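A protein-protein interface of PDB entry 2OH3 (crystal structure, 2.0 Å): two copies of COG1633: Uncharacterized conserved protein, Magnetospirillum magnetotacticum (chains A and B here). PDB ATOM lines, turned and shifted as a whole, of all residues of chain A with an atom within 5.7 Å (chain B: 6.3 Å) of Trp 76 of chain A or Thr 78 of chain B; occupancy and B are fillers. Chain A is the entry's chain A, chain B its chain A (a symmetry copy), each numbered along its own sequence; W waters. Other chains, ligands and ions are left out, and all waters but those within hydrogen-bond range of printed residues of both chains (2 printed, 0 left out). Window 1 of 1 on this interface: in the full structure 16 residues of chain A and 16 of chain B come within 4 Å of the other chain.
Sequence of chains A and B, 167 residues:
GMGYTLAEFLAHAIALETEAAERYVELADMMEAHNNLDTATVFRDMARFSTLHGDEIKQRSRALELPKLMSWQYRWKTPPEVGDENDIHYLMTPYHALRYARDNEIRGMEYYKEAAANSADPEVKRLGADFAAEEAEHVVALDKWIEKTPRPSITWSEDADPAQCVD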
ATOM      1  N   LEU A  16       5.301   1.894  -4.937  1.00  0.00           N
ATOM      2  CA  LEU A  16       5.008   1.476  -3.560  1.00  0.00           C
ATOM      3  C   LEU A  16       5.147  -0.020  -3.406  1.00  0.00           C
ATOM      4  O   LEU A  16       5.663  -0.488  -2.401  1.00  0.00           O
ATOM      5  CB  LEU A  16       3.606   1.909  -3.087  1.00  0.00           C
ATOM      6  CG  LEU A  16       3.431   3.411  -2.761  1.00  0.00           C
ATOM      7  CD1 LEU A  16       1.952   3.836  -2.599  1.00  0.00           C
ATOM      8  CD2 LEU A  16       4.244   3.852  -1.522  1.00  0.00           C
ATOM      9  N   GLU A  19       8.856  -1.223  -3.919  1.00  0.00           N
ATOM     10  CA  GLU A  19       9.496  -0.933  -2.659  1.00  0.00           C
ATOM     11  C   GLU A  19       9.082  -1.964  -1.607  1.00  0.00           C
ATOM     12  O   GLU A  19       9.939  -2.531  -0.977  1.00  0.00           O
ATOM     13  CB  GLU A  19       9.198   0.506  -2.201  1.00  0.00           C
ATOM     14  CG  GLU A  19       9.679   0.819  -0.789  1.00  0.00           C
ATOM     15  CD  GLU A  19      11.186   1.075  -0.669  1.00  0.00           C
ATOM     16  OE1 GLU A  19      11.943   0.869  -1.629  1.00  0.00           O
ATOM     17  OE2 GLU A  19      11.642   1.537   0.411  1.00  0.00           O
ATOM     18  N   ALA A  20       7.790  -2.215  -1.416  1.00  0.00           N
ATOM     19  CA  ALA A  20       7.337  -3.178  -0.408  1.00  0.00           C
ATOM     20  C   ALA A  20       7.945  -4.562  -0.599  1.00  0.00           C
ATOM     21  O   ALA A  20       8.404  -5.177   0.352  1.00  0.00           O
ATOM     22  CB  ALA A  20       5.841  -3.281  -0.372  1.00  0.00           C
ATOM     23  N   ARG A  23      11.569  -4.490   0.608  1.00  0.00           N
ATOM     24  CA  ARG A  23      11.724  -4.254   2.048  1.00  0.00           C
ATOM     25  C   ARG A  23      11.301  -5.467   2.883  1.00  0.00           C
ATOM     26  O   ARG A  23      11.911  -5.784   3.908  1.00  0.00           O
ATOM     27  CB  ARG A  23      10.896  -3.073   2.496  1.00  0.00           C
ATOM     28  CG  ARG A  23      11.288  -1.689   1.928  1.00  0.00           C
ATOM     29  CD  ARG A  23      12.541  -1.109   2.499  1.00  0.00           C
ATOM     30  NE  ARG A  23      13.732  -1.836   2.095  1.00  0.00           N
ATOM     31  CZ  ARG A  23      14.212  -1.954   0.862  1.00  0.00           C
ATOM     32  NH1 ARG A  23      13.654  -1.374  -0.181  1.00  0.00           N
ATOM     33  NH2 ARG A  23      15.306  -2.667   0.668  1.00  0.00           N
ATOM     34  N   TYR A  24      10.192  -6.068   2.484  1.00  0.00           N
ATOM     35  CA  TYR A  24       9.740  -7.342   3.070  1.00  0.00           C
ATOM     36  C   TYR A  24      10.651  -8.542   2.860  1.00  0.00           C
ATOM     37  O   TYR A  24      10.785  -9.325   3.772  1.00  0.00           O
ATOM     38  CB  TYR A  24       8.337  -7.659   2.613  1.00  0.00           C
ATOM     39  CG  TYR A  24       7.265  -6.902   3.374  1.00  0.00           C
ATOM     40  CD1 TYR A  24       7.120  -7.081   4.740  1.00  0.00           C
ATOM     41  CD2 TYR A  24       6.368  -6.077   2.726  1.00  0.00           C
ATOM     42  CE1 TYR A  24       6.156  -6.410   5.457  1.00  0.00           C
ATOM     43  CE2 TYR A  24       5.348  -5.443   3.420  1.00  0.00           C
ATOM     44  CZ  TYR A  24       5.284  -5.588   4.806  1.00  0.00           C
ATOM     45  OH  TYR A  24       4.318  -4.986   5.557  1.00  0.00           O
ATOM     46  N   LEU A  27      13.352  -7.913   5.381  1.00  0.00           N
ATOM     47  CA  LEU A  27      12.907  -8.240   6.725  1.00  0.00           C
ATOM     48  C   LEU A  27      12.725  -9.756   6.934  1.00  0.00           C
ATOM     49  O   LEU A  27      13.083 -10.271   8.000  1.00  0.00           O
ATOM     50  CB  LEU A  27      11.602  -7.489   7.090  1.00  0.00           C
ATOM     51  CG  LEU A  27      11.600  -5.958   7.194  1.00  0.00           C
ATOM     52  CD1 LEU A  27      10.169  -5.497   7.336  1.00  0.00           C
ATOM     53  CD2 LEU A  27      12.443  -5.453   8.352  1.00  0.00           C
ATOM     54  N   TYR A  74       7.972   7.398  -2.564  1.00  0.00           N
ATOM     55  CA  TYR A  74       7.535   6.003  -2.448  1.00  0.00           C
ATOM     56  C   TYR A  74       8.376   5.159  -1.490  1.00  0.00           C
ATOM     57  O   TYR A  74       7.885   4.163  -1.020  1.00  0.00           O
ATOM     58  CB  TYR A  74       7.424   5.328  -3.843  1.00  0.00           C
ATOM     59  CG  TYR A  74       8.774   5.250  -4.535  1.00  0.00           C
ATOM     60  CD1 TYR A  74       9.670   4.237  -4.207  1.00  0.00           C
ATOM     61  CD2 TYR A  74       9.194   6.230  -5.455  1.00  0.00           C
ATOM     62  CE1 TYR A  74      10.906   4.179  -4.764  1.00  0.00           C
ATOM     63  CE2 TYR A  74      10.467   6.147  -6.047  1.00  0.00           C
ATOM     64  CZ  TYR A  74      11.299   5.107  -5.674  1.00  0.00           C
ATOM     65  OH  TYR A  74      12.549   4.954  -6.177  1.00  0.00           O
ATOM     66  N   ARG A  75       9.625   5.534  -1.216  1.00  0.00           N
ATOM     67  CA  ARG A  75      10.464   4.744  -0.297  1.00  0.00           C
ATOM     68  C   ARG A  75       9.870   4.658   1.116  1.00  0.00           C
ATOM     69  O   ARG A  75       9.343   5.627   1.645  1.00  0.00           O
ATOM     70  CB  ARG A  75      11.865   5.305  -0.197  1.00  0.00           C
ATOM     71  CG  ARG A  75      12.762   4.959  -1.336  1.00  0.00           C
ATOM     72  CD  ARG A  75      14.127   5.480  -1.061  1.00  0.00           C
ATOM     73  NE  ARG A  75      15.088   4.939  -2.010  1.00  0.00           N
ATOM     74  CZ  ARG A  75      16.389   5.103  -1.911  1.00  0.00           C
ATOM     75  NH1 ARG A  75      16.883   5.879  -0.982  1.00  0.00           N
ATOM     76  NH2 ARG A  75      17.195   4.563  -2.810  1.00  0.00           N
ATOM     77  N   TRP A  76      10.008   3.501   1.751  1.00  0.00           N
ATOM     78  CA  TRP A  76       9.793   3.418   3.194  1.00  0.00           C
ATOM     79  C   TRP A  76      10.673   4.400   3.942  1.00  0.00           C
ATOM     80  O   TRP A  76      11.807   4.706   3.519  1.00  0.00           O
ATOM     81  CB  TRP A  76      10.057   1.996   3.691  1.00  0.00           C
ATOM     82  CG  TRP A  76       9.015   1.011   3.289  1.00  0.00           C
ATOM     83  CD1 TRP A  76       8.149   1.085   2.213  1.00  0.00           C
ATOM     84  CD2 TRP A  76       8.756  -0.251   3.911  1.00  0.00           C
ATOM     85  NE1 TRP A  76       7.357  -0.045   2.166  1.00  0.00           N
ATOM     86  CE2 TRP A  76       7.725  -0.884   3.181  1.00  0.00           C
ATOM     87  CE3 TRP A  76       9.287  -0.899   5.026  1.00  0.00           C
ATOM     88  CZ2 TRP A  76       7.198  -2.110   3.546  1.00  0.00           C
ATOM     89  CZ3 TRP A  76       8.760  -2.126   5.391  1.00  0.00           C
ATOM     90  CH2 TRP A  76       7.725  -2.716   4.648  1.00  0.00           C
ATOM     91  N   LYS A  77      10.148   4.919   5.051  1.00  0.00           N
ATOM     92  CA  LYS A  77      10.870   5.857   5.918  1.00  0.00           C
ATOM     93  C   LYS A  77      12.074   5.115   6.475  1.00  0.00           C
ATOM     94  O   LYS A  77      12.029   3.925   6.659  1.00  0.00           O
ATOM     95  CB  LYS A  77       9.956   6.334   7.064  1.00  0.00           C
ATOM     96  CG  LYS A  77      10.163   7.752   7.573  1.00  0.00           C
ATOM     97  CD  LYS A  77       9.769   7.894   9.095  1.00  0.00           C
ATOM     98  CE  LYS A  77       9.985   9.309   9.672  1.00  0.00           C
ATOM     99  NZ  LYS A  77       9.154  10.417   9.036  1.00  0.00           N
ATOM    100  N   THR A  78      13.186   5.793   6.699  1.00  0.00           N
ATOM    101  CA  THR A  78      14.333   5.101   7.293  1.00  0.00           C
ATOM    102  C   THR A  78      13.952   4.836   8.764  1.00  0.00           C
ATOM    103  O   THR A  78      13.286   5.663   9.387  1.00  0.00           O
ATOM    104  CB  THR A  78      15.684   5.897   7.163  1.00  0.00           C
ATOM    105  OG1 THR A  78      15.593   7.135   7.860  1.00  0.00           O
ATOM    106  CG2 THR A  78      16.053   6.163   5.670  1.00  0.00           C
ATOM    107  N   TYR A 100       8.020  -1.472  12.253  1.00  0.00           N
ATOM    108  CA  TYR A 100       8.593  -0.757  11.109  1.00  0.00           C
ATOM    109  C   TYR A 100       7.736  -1.044   9.873  1.00  0.00           C
ATOM    110  O   TYR A 100       7.354  -0.142   9.073  1.00  0.00           O
ATOM    111  CB  TYR A 100      10.052  -1.253  10.883  1.00  0.00           C
ATOM    112  CG  TYR A 100      10.723  -0.696   9.633  1.00  0.00           C
ATOM    113  CD1 TYR A 100      10.818   0.672   9.439  1.00  0.00           C
ATOM    114  CD2 TYR A 100      11.249  -1.536   8.663  1.00  0.00           C
ATOM    115  CE1 TYR A 100      11.402   1.202   8.307  1.00  0.00           C
ATOM    116  CE2 TYR A 100      11.851  -1.012   7.525  1.00  0.00           C
ATOM    117  CZ  TYR A 100      11.922   0.360   7.372  1.00  0.00           C
ATOM    118  OH  TYR A 100      12.523   0.912   6.271  1.00  0.00           O
ATOM    119  N   ALA A 101       7.423  -2.305   9.700  1.00  0.00           N
ATOM    120  CA  ALA A 101       6.609  -2.703   8.534  1.00  0.00           C
ATOM    121  C   ALA A 101       5.239  -2.060   8.615  1.00  0.00           C
ATOM    122  O   ALA A 101       4.746  -1.467   7.667  1.00  0.00           O
ATOM    123  CB  ALA A 101       6.459  -4.239   8.465  1.00  0.00           C
ATOM    124  N   ASN A 104       5.071   1.725   7.618  1.00  0.00           N
ATOM    125  CA  ASN A 104       5.085   1.919   6.192  1.00  0.00           C
ATOM    126  C   ASN A 104       3.866   1.403   5.443  1.00  0.00           C
ATOM    127  O   ASN A 104       3.498   1.964   4.432  1.00  0.00           O
ATOM    128  CB  ASN A 104       6.406   1.398   5.677  1.00  0.00           C
ATOM    129  CG  ASN A 104       7.530   2.231   6.166  1.00  0.00           C
ATOM    130  OD1 ASN A 104       7.678   3.351   5.708  1.00  0.00           O
ATOM    131  ND2 ASN A 104       8.300   1.733   7.161  1.00  0.00           N
ATOM    132  N   GLU A 105       3.216   0.357   5.950  1.00  0.00           N
ATOM    133  CA  GLU A 105       1.915  -0.062   5.456  1.00  0.00           C
ATOM    134  C   GLU A 105       0.930   1.071   5.594  1.00  0.00           C
ATOM    135  O   GLU A 105       0.159   1.314   4.691  1.00  0.00           O
ATOM    136  CB  GLU A 105       1.373  -1.247   6.275  1.00  0.00           C
ATOM    137  CG  GLU A 105       2.023  -2.579   6.003  1.00  0.00           C
ATOM    138  CD  GLU A 105       1.589  -3.171   4.700  1.00  0.00           C
ATOM    139  OE1 GLU A 105       0.515  -2.789   4.220  1.00  0.00           O
ATOM    140  OE2 GLU A 105       2.308  -4.024   4.151  1.00  0.00           O
ATOM    141  N   ARG B  75      21.259   3.697   2.424  1.00  0.00           N
ATOM    142  CA  ARG B  75      20.339   4.709   1.874  1.00  0.00           C
ATOM    143  C   ARG B  75      20.473   6.069   2.574  1.00  0.00           C
ATOM    144  O   ARG B  75      20.622   6.149   3.786  1.00  0.00           O
ATOM    145  CB  ARG B  75      18.898   4.262   1.962  1.00  0.00           C
ATOM    146  CG  ARG B  75      18.477   3.290   0.914  1.00  0.00           C
ATOM    147  CD  ARG B  75      17.022   3.019   1.053  1.00  0.00           C
ATOM    148  NE  ARG B  75      16.519   2.291  -0.103  1.00  0.00           N
ATOM    149  CZ  ARG B  75      15.244   2.053  -0.323  1.00  0.00           C
ATOM    150  NH1 ARG B  75      14.352   2.379   0.576  1.00  0.00           N
ATOM    151  NH2 ARG B  75      14.869   1.398  -1.408  1.00  0.00           N
ATOM    152  N   TRP B  76      20.364   7.146   1.808  1.00  0.00           N
ATOM    153  CA  TRP B  76      20.134   8.460   2.407  1.00  0.00           C
ATOM    154  C   TRP B  76      18.900   8.459   3.286  1.00  0.00           C
ATOM    155  O   TRP B  76      17.916   7.739   3.022  1.00  0.00           O
ATOM    156  CB  TRP B  76      20.000   9.526   1.318  1.00  0.00           C
ATOM    157  CG  TRP B  76      21.279   9.854   0.630  1.00  0.00           C
ATOM    158  CD1 TRP B  76      22.405   9.059   0.511  1.00  0.00           C
ATOM    159  CD2 TRP B  76      21.563  11.045  -0.108  1.00  0.00           C
ATOM    160  NE1 TRP B  76      23.368   9.714  -0.230  1.00  0.00           N
ATOM    161  CE2 TRP B  76      22.868  10.921  -0.636  1.00  0.00           C
ATOM    162  CE3 TRP B  76      20.845  12.213  -0.360  1.00  0.00           C
ATOM    163  CZ2 TRP B  76      23.475  11.925  -1.369  1.00  0.00           C
ATOM    164  CZ3 TRP B  76      21.451  13.219  -1.094  1.00  0.00           C
ATOM    165  CH2 TRP B  76      22.756  13.062  -1.589  1.00  0.00           C
ATOM    166  N   LYS B  77      18.951   9.253   4.355  1.00  0.00           N
ATOM    167  CA  LYS B  77      17.835   9.404   5.296  1.00  0.00           C
ATOM    168  C   LYS B  77      16.678  10.016   4.524  1.00  0.00           C
ATOM    169  O   LYS B  77      16.885  10.759   3.598  1.00  0.00           O
ATOM    170  CB  LYS B  77      18.246  10.322   6.465  1.00  0.00           C
ATOM    171  CG  LYS B  77      17.632  10.031   7.826  1.00  0.00           C
ATOM    172  CD  LYS B  77      17.503  11.336   8.705  1.00  0.00           C
ATOM    173  CE  LYS B  77      16.860  11.102  10.088  1.00  0.00           C
ATOM    174  NZ  LYS B  77      17.626  10.176  11.025  1.00  0.00           N
ATOM    175  N   THR B  78      15.446   9.672   4.853  1.00  0.00           N
ATOM    176  CA  THR B  78      14.322  10.302   4.157  1.00  0.00           C
ATOM    177  C   THR B  78      14.272  11.758   4.662  1.00  0.00           C
ATOM    178  O   THR B  78      14.548  12.014   5.834  1.00  0.00           O
ATOM    179  CB  THR B  78      12.953   9.553   4.365  1.00  0.00           C
ATOM    180  OG1 THR B  78      12.593   9.565   5.742  1.00  0.00           O
ATOM    181  CG2 THR B  78      13.020   8.080   3.855  1.00  0.00           C
ATOM    182  N   PRO B  79      13.941  12.708   3.782  1.00  0.00           N
ATOM    183  CA  PRO B  79      13.935  14.128   4.155  1.00  0.00           C
ATOM    184  C   PRO B  79      12.716  14.474   5.028  1.00  0.00           C
ATOM    185  O   PRO B  79      11.876  13.619   5.238  1.00  0.00           O
ATOM    186  CB  PRO B  79      13.855  14.834   2.802  1.00  0.00           C
ATOM    187  CG  PRO B  79      13.105  13.876   1.921  1.00  0.00           C
ATOM    188  CD  PRO B  79      13.548  12.502   2.373  1.00  0.00           C
ATOM    189  N   PRO B  80      12.622  15.726   5.529  1.00  0.00           N
ATOM    190  CA  PRO B  80      11.436  16.141   6.328  1.00  0.00           C
ATOM    191  C   PRO B  80      10.106  15.878   5.596  1.00  0.00           C
ATOM    192  O   PRO B  80       9.994  16.164   4.403  1.00  0.00           O
ATOM    193  CB  PRO B  80      11.657  17.644   6.557  1.00  0.00           C
ATOM    194  CG  PRO B  80      13.132  17.815   6.449  1.00  0.00           C
ATOM    195  CD  PRO B  80      13.607  16.823   5.402  1.00  0.00           C
ATOM    196  N   TYR B 100      19.902  18.903   2.561  1.00  0.00           N
ATOM    197  CA  TYR B 100      19.587  17.471   2.517  1.00  0.00           C
ATOM    198  C   TYR B 100      20.822  16.714   2.020  1.00  0.00           C
ATOM    199  O   TYR B 100      21.258  15.664   2.574  1.00  0.00           O
ATOM    200  CB  TYR B 100      18.389  17.248   1.548  1.00  0.00           C
ATOM    201  CG  TYR B 100      18.045  15.785   1.295  1.00  0.00           C
ATOM    202  CD1 TYR B 100      17.762  14.938   2.353  1.00  0.00           C
ATOM    203  CD2 TYR B 100      18.010  15.265   0.009  1.00  0.00           C
ATOM    204  CE1 TYR B 100      17.468  13.604   2.153  1.00  0.00           C
ATOM    205  CE2 TYR B 100      17.702  13.926  -0.204  1.00  0.00           C
ATOM    206  CZ  TYR B 100      17.428  13.117   0.882  1.00  0.00           C
ATOM    207  OH  TYR B 100      17.105  11.797   0.708  1.00  0.00           O
ATOM    208  N   ASN B 104      23.489  13.940   4.266  1.00  0.00           N
ATOM    209  CA  ASN B 104      23.880  12.624   3.832  1.00  0.00           C
ATOM    210  C   ASN B 104      25.344  12.461   3.454  1.00  0.00           C
ATOM    211  O   ASN B 104      25.895  11.394   3.625  1.00  0.00           O
ATOM    212  CB  ASN B 104      22.903  12.192   2.763  1.00  0.00           C
ATOM    213  CG  ASN B 104      21.550  11.996   3.333  1.00  0.00           C
ATOM    214  OD1 ASN B 104      21.344  11.034   4.052  1.00  0.00           O
ATOM    215  ND2 ASN B 104      20.616  12.945   3.085  1.00  0.00           N
HETATM  216  O   HOH W   1      15.700   7.118   1.205  1.00  0.00           O
HETATM  217  O   HOH W   2      14.550   3.867   2.914  1.00  0.00           O
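Printed residues of chain B within 4 Å of Glu 19 of chain A: Arg 75 (2.8 Å).
Of the printed residues of chain B, Trp 76 of chain A touches Thr 78.
Of the printed residues of chain B, Thr 78 of chain A touches Trp 76, Lys 77 and Thr 78.
Ala 101 of chain A touches none of the printed residues of chain B.
Asn 104 of chain A touches none of the printed residues of chain B.
Of the printed residues of chain A, Arg 75 of chain B touches Glu 19 (2.8 Å), Arg 23 (3.3 Å) and Arg 75 (3.3 Å).
Of chain A, only Trp 76 (3.6 Å), Lys 77 (3.5 Å) and Thr 78 (3.7 Å) come within 4 Å of Thr 78 of chain B.
The nearest residue of chain B that does not touch Trp 76 of chain A is Arg 75 of chain B (4.5 Å).
Among the printed residues, pairs that only touch across the chains: Arg 75 of chain A with Arg 75 of chain B (3.3 Å), Trp 76 of chain A with Thr 78 of chain B (3.6 Å), Lys 77 of chain A with Thr 78 of chain B (3.5 Å), Thr 78 of chain A with Trp 76 of chain B (3.6 Å), Thr 78 of chain A with Lys 77 of chain B (3.5 Å) and Thr 78 of chain A with Thr 78 of chain B (3.7 Å).
The side-chain carboxylate (OE1) of Glu 19 of chain A lies within salt-bridge range of the guanidinium group (NH1) of Arg 23 of chain A, at 3.2 Å.
The side-chain carboxylate (OE2) of Glu 19 of chain A lies within hydrogen-bond range of the backbone NH (N) of Trp 76 of chain A, 2.9 Å away.
The backbone NH (N) of Lys 77 of chain B lies within hydrogen-bond range of the side-chain amide oxygen (OD1) of Asn 104 of chain B (3.0 Å).
The backbone carbonyl oxygen (O) of Lys 77 of chain A is in hydrogen-bond range of the side-chain hydroxyl (OH) of Tyr 100 of chain A.
N of Lys 77 of chain A lies within hydrogen-bond range of OD1 of Asn 104 of chain A, at 3.0 Å.
The side-chain hydroxyl of Tyr 100 of chain B is in hydrogen-bond range of the backbone carbonyl oxygen of Lys 77 of chain B, 3.1 Å away.
Water W1 lies within hydrogen-bond range of NH1 of Arg 75 of chain A (2.8 Å) and O of Trp 76 of chain B (2.9 Å).
Water W2 lies within hydrogen-bond range of the guanidinium group (NH1) of Arg 75 of chain B and the backbone carbonyl oxygen (O) of Trp 76 of chain A.
Printed residues of chain B that touch a printed residue of chain A: Arg 75, Trp 76, Lys 77 and Thr 78.
Along chain B the printed residues that touch a printed residue of chain A span positions 75 to 78.
Of the 15 printed residues of chain A, 6 touch a printed residue of chain B.
Among the printed residues, 8 pairs touch across the chains.
Arg 75 of chain A touches its own counterpart, Arg 75 of chain B.
Trp 76 of chain A touches Thr 78 of chain B, and with the chains exchanged Thr 78 of chain A touches Trp 76 of chain B.
Lys 77 of chain A touches Thr 78 of chain B, and with the chains exchanged Thr 78 of chain A touches Lys 77 of chain B.
Thr 78 of chain A touches its own counterpart, Thr 78 of chain B.
Positions printed for both chains: 75, 76, 77, 78, 100 and 104.
Of the 8 pairs that touch across the chains among the printed residues, 6 have their exchanged pair printed and touching as well.
OE2 of Glu 19 of chain A lies within salt-bridge range of NH1 of Arg 75 of chain B (2.8 Å).
The guanidinium group (NH1) of Arg 23 of chain A lies close to the guanidinium group (NH2) of Arg 75 of chain B (3.3 Å).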
